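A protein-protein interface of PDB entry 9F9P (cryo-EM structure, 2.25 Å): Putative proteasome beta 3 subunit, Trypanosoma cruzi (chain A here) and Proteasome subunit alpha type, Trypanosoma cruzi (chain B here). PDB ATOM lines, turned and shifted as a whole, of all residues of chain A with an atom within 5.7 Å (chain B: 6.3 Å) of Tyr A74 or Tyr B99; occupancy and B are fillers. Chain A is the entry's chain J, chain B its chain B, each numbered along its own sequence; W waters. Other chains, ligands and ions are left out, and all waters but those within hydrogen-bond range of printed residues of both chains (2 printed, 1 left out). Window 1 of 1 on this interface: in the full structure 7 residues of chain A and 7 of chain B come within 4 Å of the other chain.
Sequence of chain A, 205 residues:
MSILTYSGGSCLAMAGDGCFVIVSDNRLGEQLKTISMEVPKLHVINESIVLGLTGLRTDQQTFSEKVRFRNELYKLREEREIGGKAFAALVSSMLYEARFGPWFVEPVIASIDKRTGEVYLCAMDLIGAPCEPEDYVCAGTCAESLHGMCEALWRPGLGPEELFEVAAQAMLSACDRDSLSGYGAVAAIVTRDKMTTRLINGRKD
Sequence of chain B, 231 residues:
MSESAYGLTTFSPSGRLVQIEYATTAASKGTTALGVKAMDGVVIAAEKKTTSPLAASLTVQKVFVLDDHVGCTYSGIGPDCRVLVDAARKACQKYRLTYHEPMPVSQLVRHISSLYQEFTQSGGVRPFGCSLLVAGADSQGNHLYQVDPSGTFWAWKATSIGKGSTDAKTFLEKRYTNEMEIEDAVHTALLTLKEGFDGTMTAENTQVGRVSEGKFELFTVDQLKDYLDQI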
ATOM      1  N   PHE A  69     -18.140  -0.330  -7.374  1.00  0.00           N
ATOM      2  CA  PHE A  69     -17.178  -0.894  -6.432  1.00  0.00           C
ATOM      3  C   PHE A  69     -17.827  -1.982  -5.560  1.00  0.00           C
ATOM      4  O   PHE A  69     -17.284  -3.065  -5.473  1.00  0.00           O
ATOM      5  CB  PHE A  69     -16.566   0.261  -5.614  1.00  0.00           C
ATOM      6  CG  PHE A  69     -15.701  -0.072  -4.420  1.00  0.00           C
ATOM      7  CD1 PHE A  69     -16.159   0.147  -3.125  1.00  0.00           C
ATOM      8  CD2 PHE A  69     -14.470  -0.680  -4.556  1.00  0.00           C
ATOM      9  CE1 PHE A  69     -15.390  -0.201  -2.016  1.00  0.00           C
ATOM     10  CE2 PHE A  69     -13.682  -0.990  -3.456  1.00  0.00           C
ATOM     11  CZ  PHE A  69     -14.120  -0.720  -2.188  1.00  0.00           C
ATOM     12  N   ARG A  70     -18.993  -1.732  -4.963  1.00  0.00           N
ATOM     13  CA  ARG A  70     -19.691  -2.736  -4.174  1.00  0.00           C
ATOM     14  C   ARG A  70     -20.100  -3.946  -5.010  1.00  0.00           C
ATOM     15  O   ARG A  70     -20.109  -5.053  -4.498  1.00  0.00           O
ATOM     16  CB  ARG A  70     -21.005  -2.252  -3.558  1.00  0.00           C
ATOM     17  CG  ARG A  70     -20.931  -1.062  -2.627  1.00  0.00           C
ATOM     18  CD  ARG A  70     -20.472  -1.389  -1.245  1.00  0.00           C
ATOM     19  NE  ARG A  70     -21.235  -0.563  -0.312  1.00  0.00           N
ATOM     20  CZ  ARG A  70     -22.187  -1.026   0.502  1.00  0.00           C
ATOM     21  NH1 ARG A  70     -22.848  -0.173   1.272  1.00  0.00           N
ATOM     22  NH2 ARG A  70     -22.481  -2.324   0.535  1.00  0.00           N
ATOM     23  N   ASN A  71     -20.498  -3.716  -6.249  1.00  0.00           N
ATOM     24  CA  ASN A  71     -20.913  -4.774  -7.135  1.00  0.00           C
ATOM     25  C   ASN A  71     -19.725  -5.666  -7.474  1.00  0.00           C
ATOM     26  O   ASN A  71     -19.899  -6.852  -7.437  1.00  0.00           O
ATOM     27  CB  ASN A  71     -21.629  -4.226  -8.366  1.00  0.00           C
ATOM     28  CG  ASN A  71     -22.046  -5.276  -9.379  1.00  0.00           C
ATOM     29  OD1 ASN A  71     -22.807  -6.195  -9.096  1.00  0.00           O
ATOM     30  ND2 ASN A  71     -21.598  -5.130 -10.608  1.00  0.00           N
ATOM     31  N   GLU A  72     -18.526  -5.113  -7.710  1.00  0.00           N
ATOM     32  CA  GLU A  72     -17.331  -5.908  -7.966  1.00  0.00           C
ATOM     33  C   GLU A  72     -16.960  -6.800  -6.781  1.00  0.00           C
ATOM     34  O   GLU A  72     -16.717  -7.975  -6.964  1.00  0.00           O
ATOM     35  CB  GLU A  72     -16.099  -5.074  -8.309  1.00  0.00           C
ATOM     36  CG  GLU A  72     -16.080  -4.505  -9.744  1.00  0.00           C
ATOM     37  CD  GLU A  72     -16.445  -5.391 -10.955  1.00  0.00           C
ATOM     38  OE1 GLU A  72     -17.206  -4.900 -11.846  1.00  0.00           O
ATOM     39  OE2 GLU A  72     -15.977  -6.570 -11.042  1.00  0.00           O
ATOM     40  N   LEU A  73     -16.986  -6.266  -5.567  1.00  0.00           N
ATOM     41  CA  LEU A  73     -16.739  -7.110  -4.423  1.00  0.00           C
ATOM     42  C   LEU A  73     -17.804  -8.164  -4.182  1.00  0.00           C
ATOM     43  O   LEU A  73     -17.485  -9.181  -3.607  1.00  0.00           O
ATOM     44  CB  LEU A  73     -16.634  -6.283  -3.159  1.00  0.00           C
ATOM     45  CG  LEU A  73     -15.481  -5.296  -3.124  1.00  0.00           C
ATOM     46  CD1 LEU A  73     -15.650  -4.491  -1.862  1.00  0.00           C
ATOM     47  CD2 LEU A  73     -14.113  -5.970  -3.168  1.00  0.00           C
ATOM     48  N   TYR A  74     -19.051  -7.908  -4.540  1.00  0.00           N
ATOM     49  CA  TYR A  74     -20.132  -8.879  -4.406  1.00  0.00           C
ATOM     50  C   TYR A  74     -19.846 -10.100  -5.270  1.00  0.00           C
ATOM     51  O   TYR A  74     -19.899 -11.194  -4.786  1.00  0.00           O
ATOM     52  CB  TYR A  74     -21.470  -8.228  -4.754  1.00  0.00           C
ATOM     53  CG  TYR A  74     -22.707  -9.079  -4.664  1.00  0.00           C
ATOM     54  CD1 TYR A  74     -23.089  -9.929  -5.685  1.00  0.00           C
ATOM     55  CD2 TYR A  74     -23.545  -9.002  -3.577  1.00  0.00           C
ATOM     56  CE1 TYR A  74     -24.199 -10.747  -5.585  1.00  0.00           C
ATOM     57  CE2 TYR A  74     -24.714  -9.733  -3.498  1.00  0.00           C
ATOM     58  CZ  TYR A  74     -25.061 -10.600  -4.507  1.00  0.00           C
ATOM     59  OH  TYR A  74     -26.236 -11.329  -4.386  1.00  0.00           O
ATOM     60  N   LYS A  75     -19.591  -9.896  -6.531  1.00  0.00           N
ATOM     61  CA  LYS A  75     -19.259 -10.969  -7.439  1.00  0.00           C
ATOM     62  C   LYS A  75     -18.097 -11.845  -6.981  1.00  0.00           C
ATOM     63  O   LYS A  75     -18.170 -13.035  -7.218  1.00  0.00           O
ATOM     64  CB  LYS A  75     -18.891 -10.389  -8.807  1.00  0.00           C
ATOM     65  CG  LYS A  75     -20.083  -9.823  -9.554  1.00  0.00           C
ATOM     66  CD  LYS A  75     -19.770  -9.427 -10.979  1.00  0.00           C
ATOM     67  CE  LYS A  75     -19.545  -7.930 -11.071  1.00  0.00           C
ATOM     68  NZ  LYS A  75     -18.753  -7.571 -12.270  1.00  0.00           N
ATOM     69  N   LEU A  76     -17.045 -11.305  -6.339  1.00  0.00           N
ATOM     70  CA  LEU A  76     -15.930 -12.134  -5.876  1.00  0.00           C
ATOM     71  C   LEU A  76     -16.321 -12.931  -4.632  1.00  0.00           C
ATOM     72  O   LEU A  76     -16.109 -14.118  -4.565  1.00  0.00           O
ATOM     73  CB  LEU A  76     -14.704 -11.265  -5.596  1.00  0.00           C
ATOM     74  CG  LEU A  76     -14.106 -10.519  -6.778  1.00  0.00           C
ATOM     75  CD1 LEU A  76     -13.203  -9.397  -6.342  1.00  0.00           C
ATOM     76  CD2 LEU A  76     -13.292 -11.443  -7.627  1.00  0.00           C
ATOM     77  N   ARG A  77     -16.939 -12.298  -3.652  1.00  0.00           N
ATOM     78  CA  ARG A  77     -17.481 -13.014  -2.505  1.00  0.00           C
ATOM     79  C   ARG A  77     -18.512 -14.058  -2.925  1.00  0.00           C
ATOM     80  O   ARG A  77     -18.388 -15.184  -2.525  1.00  0.00           O
ATOM     81  CB  ARG A  77     -18.172 -12.087  -1.515  1.00  0.00           C
ATOM     82  CG  ARG A  77     -17.293 -11.166  -0.689  1.00  0.00           C
ATOM     83  CD  ARG A  77     -18.190 -10.678   0.469  1.00  0.00           C
ATOM     84  NE  ARG A  77     -19.479 -10.070   0.096  1.00  0.00           N
ATOM     85  CZ  ARG A  77     -19.648  -8.781  -0.265  1.00  0.00           C
ATOM     86  NH1 ARG A  77     -18.624  -7.954  -0.298  1.00  0.00           N
ATOM     87  NH2 ARG A  77     -20.840  -8.312  -0.593  1.00  0.00           N
ATOM     88  N   GLU A  78     -19.544 -13.722  -3.698  1.00  0.00           N
ATOM     89  CA  GLU A  78     -20.714 -14.585  -3.838  1.00  0.00           C
ATOM     90  C   GLU A  78     -20.650 -15.493  -5.062  1.00  0.00           C
ATOM     91  O   GLU A  78     -21.464 -16.398  -5.199  1.00  0.00           O
ATOM     92  CB  GLU A  78     -22.004 -13.788  -4.012  1.00  0.00           C
ATOM     93  CG  GLU A  78     -22.342 -12.838  -2.866  1.00  0.00           C
ATOM     94  CD  GLU A  78     -23.716 -12.979  -2.196  1.00  0.00           C
ATOM     95  OE1 GLU A  78     -24.004 -12.163  -1.264  1.00  0.00           O
ATOM     96  OE2 GLU A  78     -24.473 -13.921  -2.526  1.00  0.00           O
ATOM     97  N   GLU A  79     -19.742 -15.187  -5.984  1.00  0.00           N
ATOM     98  CA  GLU A  79     -19.609 -15.932  -7.221  1.00  0.00           C
ATOM     99  C   GLU A  79     -20.917 -16.036  -8.011  1.00  0.00           C
ATOM    100  O   GLU A  79     -21.186 -17.079  -8.593  1.00  0.00           O
ATOM    101  CB  GLU A  79     -19.019 -17.303  -6.937  1.00  0.00           C
ATOM    102  CG  GLU A  79     -17.762 -17.218  -6.097  1.00  0.00           C
ATOM    103  CD  GLU A  79     -16.876 -18.463  -5.941  1.00  0.00           C
ATOM    104  OE1 GLU A  79     -15.847 -18.348  -5.224  1.00  0.00           O
ATOM    105  OE2 GLU A  79     -17.197 -19.540  -6.493  1.00  0.00           O
ATOM    106  N   ARG A  80     -21.641 -14.932  -8.142  1.00  0.00           N
ATOM    107  CA  ARG A  80     -22.833 -14.869  -8.967  1.00  0.00           C
ATOM    108  C   ARG A  80     -23.127 -13.403  -9.260  1.00  0.00           C
ATOM    109  O   ARG A  80     -22.583 -12.521  -8.589  1.00  0.00           O
ATOM    110  CB  ARG A  80     -24.027 -15.549  -8.285  1.00  0.00           C
ATOM    111  CG  ARG A  80     -24.416 -14.901  -6.970  1.00  0.00           C
ATOM    112  CD  ARG A  80     -25.669 -15.465  -6.285  1.00  0.00           C
ATOM    113  NE  ARG A  80     -25.956 -14.812  -5.005  1.00  0.00           N
ATOM    114  CZ  ARG A  80     -27.165 -14.733  -4.487  1.00  0.00           C
ATOM    115  NH1 ARG A  80     -28.182 -15.182  -5.179  1.00  0.00           N
ATOM    116  NH2 ARG A  80     -27.395 -14.208  -3.291  1.00  0.00           N
ATOM    117  N   GLU A  81     -23.936 -13.132 -10.282  1.00  0.00           N
ATOM    118  CA  GLU A  81     -24.446 -11.785 -10.538  1.00  0.00           C
ATOM    119  C   GLU A  81     -25.582 -11.454  -9.579  1.00  0.00           C
ATOM    120  O   GLU A  81     -26.363 -12.323  -9.234  1.00  0.00           O
ATOM    121  CB  GLU A  81     -25.002 -11.690 -11.956  1.00  0.00           C
ATOM    122  CG  GLU A  81     -23.961 -11.944 -13.038  1.00  0.00           C
ATOM    123  CD  GLU A  81     -22.900 -10.851 -13.228  1.00  0.00           C
ATOM    124  OE1 GLU A  81     -21.968 -11.070 -14.040  1.00  0.00           O
ATOM    125  OE2 GLU A  81     -23.006  -9.768 -12.587  1.00  0.00           O
ATOM    126  N   ILE A  82     -25.670 -10.198  -9.142  1.00  0.00           N
ATOM    127  CA  ILE A  82     -26.770  -9.763  -8.301  1.00  0.00           C
ATOM    128  C   ILE A  82     -28.041  -9.632  -9.136  1.00  0.00           C
ATOM    129  O   ILE A  82     -27.978  -9.360 -10.334  1.00  0.00           O
ATOM    130  CB  ILE A  82     -26.389  -8.461  -7.599  1.00  0.00           C
ATOM    131  CG1 ILE A  82     -27.346  -8.104  -6.464  1.00  0.00           C
ATOM    132  CG2 ILE A  82     -26.279  -7.319  -8.595  1.00  0.00           C
ATOM    133  CD1 ILE A  82     -26.749  -7.057  -5.501  1.00  0.00           C
ATOM    134  N   GLY A  83     -29.189  -9.907  -8.527  1.00  0.00           N
ATOM    135  CA  GLY A  83     -30.483  -9.737  -9.170  1.00  0.00           C
ATOM    136  C   GLY A  83     -31.143  -8.405  -8.811  1.00  0.00           C
ATOM    137  O   GLY A  83     -30.802  -7.764  -7.824  1.00  0.00           O
ATOM    138  N   LYS A  85     -34.041  -7.222  -7.489  1.00  0.00           N
ATOM    139  CA  LYS A  85     -34.593  -6.869  -6.189  1.00  0.00           C
ATOM    140  C   LYS A  85     -33.498  -6.696  -5.150  1.00  0.00           C
ATOM    141  O   LYS A  85     -33.591  -5.810  -4.293  1.00  0.00           O
ATOM    142  CB  LYS A  85     -35.583  -7.914  -5.686  1.00  0.00           C
ATOM    143  CG  LYS A  85     -37.048  -7.637  -5.982  1.00  0.00           C
ATOM    144  CD  LYS A  85     -37.790  -8.854  -6.513  1.00  0.00           C
ATOM    145  CE  LYS A  85     -39.227  -8.567  -6.918  1.00  0.00           C
ATOM    146  NZ  LYS A  85     -39.672  -9.429  -8.051  1.00  0.00           N
ATOM    147  N   ALA A  86     -32.442  -7.505  -5.208  1.00  0.00           N
ATOM    148  CA  ALA A  86     -31.374  -7.307  -4.245  1.00  0.00           C
ATOM    149  C   ALA A  86     -30.543  -6.066  -4.525  1.00  0.00           C
ATOM    150  O   ALA A  86     -30.052  -5.425  -3.612  1.00  0.00           O
ATOM    151  CB  ALA A  86     -30.519  -8.523  -4.173  1.00  0.00           C
ATOM    152  N   ALA A  89     -32.520  -2.979  -3.128  1.00  0.00           N
ATOM    153  CA  ALA A  89     -32.372  -2.952  -1.686  1.00  0.00           C
ATOM    154  C   ALA A  89     -31.007  -2.464  -1.264  1.00  0.00           C
ATOM    155  O   ALA A  89     -30.913  -1.652  -0.362  1.00  0.00           O
ATOM    156  CB  ALA A  89     -32.625  -4.325  -1.147  1.00  0.00           C
ATOM    157  N   LEU A  90     -29.964  -2.897  -1.977  1.00  0.00           N
ATOM    158  CA  LEU A  90     -28.634  -2.360  -1.728  1.00  0.00           C
ATOM    159  C   LEU A  90     -28.587  -0.854  -1.937  1.00  0.00           C
ATOM    160  O   LEU A  90     -28.113  -0.146  -1.081  1.00  0.00           O
ATOM    161  CB  LEU A  90     -27.615  -3.074  -2.608  1.00  0.00           C
ATOM    162  CG  LEU A  90     -26.199  -2.489  -2.619  1.00  0.00           C
ATOM    163  CD1 LEU A  90     -25.542  -2.629  -1.286  1.00  0.00           C
ATOM    164  CD2 LEU A  90     -25.327  -3.203  -3.617  1.00  0.00           C
ATOM    165  N   LYS B  94     -28.342  -9.226   9.497  1.00  0.00           N
ATOM    166  CA  LYS B  94     -27.666  -8.144   8.819  1.00  0.00           C
ATOM    167  C   LYS B  94     -27.707  -8.288   7.296  1.00  0.00           C
ATOM    168  O   LYS B  94     -27.903  -7.312   6.611  1.00  0.00           O
ATOM    169  CB  LYS B  94     -26.253  -8.075   9.356  1.00  0.00           C
ATOM    170  CG  LYS B  94     -25.446  -6.936   8.778  1.00  0.00           C
ATOM    171  CD  LYS B  94     -23.933  -7.113   8.936  1.00  0.00           C
ATOM    172  CE  LYS B  94     -23.159  -6.009   8.243  1.00  0.00           C
ATOM    173  NZ  LYS B  94     -21.801  -6.459   7.847  1.00  0.00           N
ATOM    174  N   TYR B  95     -27.643  -9.508   6.765  1.00  0.00           N
ATOM    175  CA  TYR B  95     -27.725  -9.745   5.343  1.00  0.00           C
ATOM    176  C   TYR B  95     -29.126  -9.465   4.795  1.00  0.00           C
ATOM    177  O   TYR B  95     -29.257  -8.888   3.726  1.00  0.00           O
ATOM    178  CB  TYR B  95     -27.340 -11.186   5.015  1.00  0.00           C
ATOM    179  CG  TYR B  95     -27.092 -11.472   3.556  1.00  0.00           C
ATOM    180  CD1 TYR B  95     -25.812 -11.419   3.019  1.00  0.00           C
ATOM    181  CD2 TYR B  95     -28.148 -11.763   2.699  1.00  0.00           C
ATOM    182  CE1 TYR B  95     -25.582 -11.736   1.690  1.00  0.00           C
ATOM    183  CE2 TYR B  95     -27.939 -12.032   1.355  1.00  0.00           C
ATOM    184  CZ  TYR B  95     -26.648 -12.044   0.852  1.00  0.00           C
ATOM    185  OH  TYR B  95     -26.482 -12.271  -0.478  1.00  0.00           O
ATOM    186  N   ARG B  96     -30.172  -9.865   5.506  1.00  0.00           N
ATOM    187  CA  ARG B  96     -31.524  -9.507   5.125  1.00  0.00           C
ATOM    188  C   ARG B  96     -31.769  -8.001   5.138  1.00  0.00           C
ATOM    189  O   ARG B  96     -32.465  -7.530   4.259  1.00  0.00           O
ATOM    190  CB  ARG B  96     -32.579 -10.127   6.044  1.00  0.00           C
ATOM    191  CG  ARG B  96     -32.930 -11.553   5.675  1.00  0.00           C
ATOM    192  CD  ARG B  96     -33.893 -12.170   6.667  1.00  0.00           C
ATOM    193  NE  ARG B  96     -33.871 -13.629   6.559  1.00  0.00           N
ATOM    194  CZ  ARG B  96     -34.532 -14.330   5.640  1.00  0.00           C
ATOM    195  NH1 ARG B  96     -34.444 -15.651   5.638  1.00  0.00           N
ATOM    196  NH2 ARG B  96     -35.287 -13.703   4.747  1.00  0.00           N
ATOM    197  N   LEU B  97     -31.269  -7.259   6.113  1.00  0.00           N
ATOM    198  CA  LEU B  97     -31.477  -5.821   6.109  1.00  0.00           C
ATOM    199  C   LEU B  97     -30.884  -5.178   4.870  1.00  0.00           C
ATOM    200  O   LEU B  97     -31.471  -4.251   4.364  1.00  0.00           O
ATOM    201  CB  LEU B  97     -30.904  -5.129   7.344  1.00  0.00           C
ATOM    202  CG  LEU B  97     -31.740  -5.336   8.606  1.00  0.00           C
ATOM    203  CD1 LEU B  97     -30.987  -4.888   9.834  1.00  0.00           C
ATOM    204  CD2 LEU B  97     -33.072  -4.597   8.557  1.00  0.00           C
ATOM    205  N   THR B  98     -29.733  -5.623   4.393  1.00  0.00           N
ATOM    206  CA  THR B  98     -29.070  -4.995   3.259  1.00  0.00           C
ATOM    207  C   THR B  98     -29.651  -5.441   1.916  1.00  0.00           C
ATOM    208  O   THR B  98     -29.866  -4.588   1.089  1.00  0.00           O
ATOM    209  CB  THR B  98     -27.581  -5.315   3.313  1.00  0.00           C
ATOM    210  OG1 THR B  98     -27.115  -4.849   4.576  1.00  0.00           O
ATOM    211  CG2 THR B  98     -26.794  -4.669   2.206  1.00  0.00           C
ATOM    212  N   TYR B  99     -29.936  -6.728   1.686  1.00  0.00           N
ATOM    213  CA  TYR B  99     -30.358  -7.230   0.382  1.00  0.00           C
ATOM    214  C   TYR B  99     -31.801  -7.751   0.320  1.00  0.00           C
ATOM    215  O   TYR B  99     -32.236  -8.178  -0.729  1.00  0.00           O
ATOM    216  CB  TYR B  99     -29.459  -8.398  -0.013  1.00  0.00           C
ATOM    217  CG  TYR B  99     -27.991  -8.075  -0.072  1.00  0.00           C
ATOM    218  CD1 TYR B  99     -27.447  -7.342  -1.128  1.00  0.00           C
ATOM    219  CD2 TYR B  99     -27.144  -8.424   0.954  1.00  0.00           C
ATOM    220  CE1 TYR B  99     -26.113  -6.953  -1.146  1.00  0.00           C
ATOM    221  CE2 TYR B  99     -25.801  -8.055   0.944  1.00  0.00           C
ATOM    222  CZ  TYR B  99     -25.278  -7.337  -0.117  1.00  0.00           C
ATOM    223  OH  TYR B  99     -23.969  -6.963  -0.077  1.00  0.00           O
ATOM    224  N   HIS B 100     -32.550  -7.784   1.419  1.00  0.00           N
ATOM    225  CA  HIS B 100     -33.923  -8.298   1.451  1.00  0.00           C
ATOM    226  C   HIS B 100     -34.071  -9.698   0.857  1.00  0.00           C
ATOM    227  O   HIS B 100     -35.066  -9.994   0.212  1.00  0.00           O
ATOM    228  CB  HIS B 100     -34.916  -7.343   0.759  1.00  0.00           C
ATOM    229  CG  HIS B 100     -35.024  -5.993   1.405  1.00  0.00           C
ATOM    230  ND1 HIS B 100     -35.632  -4.901   0.838  1.00  0.00           N
ATOM    231  CD2 HIS B 100     -34.581  -5.576   2.571  1.00  0.00           C
ATOM    232  CE1 HIS B 100     -35.536  -3.857   1.664  1.00  0.00           C
ATOM    233  NE2 HIS B 100     -34.918  -4.259   2.744  1.00  0.00           N
ATOM    234  N   GLU B 101     -33.101 -10.569   1.086  1.00  0.00           N
ATOM    235  CA  GLU B 101     -33.249 -11.968   0.767  1.00  0.00           C
ATOM    236  C   GLU B 101     -32.437 -12.795   1.764  1.00  0.00           C
ATOM    237  O   GLU B 101     -31.645 -12.269   2.498  1.00  0.00           O
ATOM    238  CB  GLU B 101     -32.883 -12.252  -0.690  1.00  0.00           C
ATOM    239  CG  GLU B 101     -31.479 -11.877  -1.088  1.00  0.00           C
ATOM    240  CD  GLU B 101     -31.077 -12.333  -2.499  1.00  0.00           C
ATOM    241  OE1 GLU B 101     -31.703 -11.873  -3.491  1.00  0.00           O
ATOM    242  OE2 GLU B 101     -30.107 -13.133  -2.617  1.00  0.00           O
ATOM    243  N   GLN B 107     -22.049 -18.159   2.042  1.00  0.00           N
ATOM    244  CA  GLN B 107     -21.560 -16.893   2.578  1.00  0.00           C
ATOM    245  C   GLN B 107     -21.553 -16.936   4.103  1.00  0.00           C
ATOM    246  O   GLN B 107     -20.716 -16.372   4.762  1.00  0.00           O
ATOM    247  CB  GLN B 107     -22.443 -15.740   2.079  1.00  0.00           C
ATOM    248  CG  GLN B 107     -22.469 -15.568   0.554  1.00  0.00           C
ATOM    249  CD  GLN B 107     -21.072 -15.422   0.010  1.00  0.00           C
ATOM    250  OE1 GLN B 107     -20.357 -14.510   0.399  1.00  0.00           O
ATOM    251  NE2 GLN B 107     -20.606 -16.379  -0.780  1.00  0.00           N
HETATM  252  O   HOH W   1     -27.966 -10.871  -2.561  1.00  0.00           O
HETATM  253  O   HOH W   2     -32.950 -10.248  -6.269  1.00  0.00           O
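Among the printed residues, merely in contact across the chains: Tyr A74 with Tyr B99 (3.9 Å), Glu A78 with Gln B107 (3.5 Å), Arg A80 with Tyr B95 (3.5 Å), Ala A86 with Tyr B99 (3.7 Å), Ala A86 with Glu B101 (3.6 Å), Ala A89 with Tyr B99 (3.8 Å), Ala A89 with His B100 (3.6 Å) and Leu A90 with Thr B98 (3.5 Å).
Of the printed residues of chain B, Arg A77 touches Tyr B99 (3.4 Å) and Gln B107 (3.1 Å). Of the printed residues of chain B, Glu A78 touches Tyr B95 (2.6 Å) and Gln B107 (3.5 Å). Gly A83 touches none of the printed residues of chain B. Printed residues of chain B within 4 Å of Ala A86: Tyr B99 and Glu B101. Of the printed residues of chain B, Ala A89 touches Thr B98 (3.4 Å), Tyr B99 (3.8 Å) and His B100 (3.6 Å). Tyr B99 touches just these residues of chain A: Tyr A74 (3.9 Å), Arg A77 (3.4 Å), Ala A86 (3.7 Å) and Ala A89 (3.8 Å). Of the printed residues of chain A, His B100 touches Ala A89 (3.6 Å). The nearest residue of chain B that does not touch Tyr A74 is Tyr B95 (4.03 Å). The nearest printed residue of chain B that does not touch Ala A89 is Leu B97 (5.4 Å).
NE2 of Gln B107 is in hydrogen-bond range of O of Arg A77 (3.1 Å). The side-chain hydroxyl (OH) of Tyr B95 is in hydrogen-bond range of the side-chain carboxylate (OE1) of Glu A78 (2.6 Å). NH2 of Arg A77 sits at hydrogen-bond distance from OH of Tyr B99 (3.4 Å). The guanidinium group (NH2) of Arg A80 is in salt-bridge range of the side-chain carboxylate (OE2) of Glu B101 (3.0 Å). O of Ala A89 sits close to O of Thr B98 (3.4 Å).
Water W1 lies within hydrogen-bond range of the side-chain hydroxyl of Tyr A74 (2.6 Å), the side-chain hydroxyl of Tyr B95 (2.9 Å), the side-chain carboxylate of Glu B101 (3.1 Å) and the guanidinium group of Arg A80 (3.5 Å). Water W2 lies within hydrogen-bond range of the backbone NH (N) of Ala A86 (3.0 Å), the backbone NH (N) of Lys A85 (3.4 Å) and the side-chain carboxylate (OE1) of Glu B101 (3.5 Å).
O of Lys B94 sits at hydrogen-bond distance from OG1 of Thr B98 (3.3 Å). OH of Tyr A74 lies within hydrogen-bond range of NH2 of Arg A80 (3.3 Å). The guanidinium group of Arg A80 is in salt-bridge range of the side-chain carboxylate of Glu A78, at 3.0 Å.
Of the 9 printed residues of chain B, 6 touch a printed residue of chain A. Of the 19 printed residues of chain A, 7 touch a printed residue of chain B. Hydrophobic or aromatic side chains of chain A that line the printed part of chain B: Tyr A74, Ala A86 and Ala A89.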
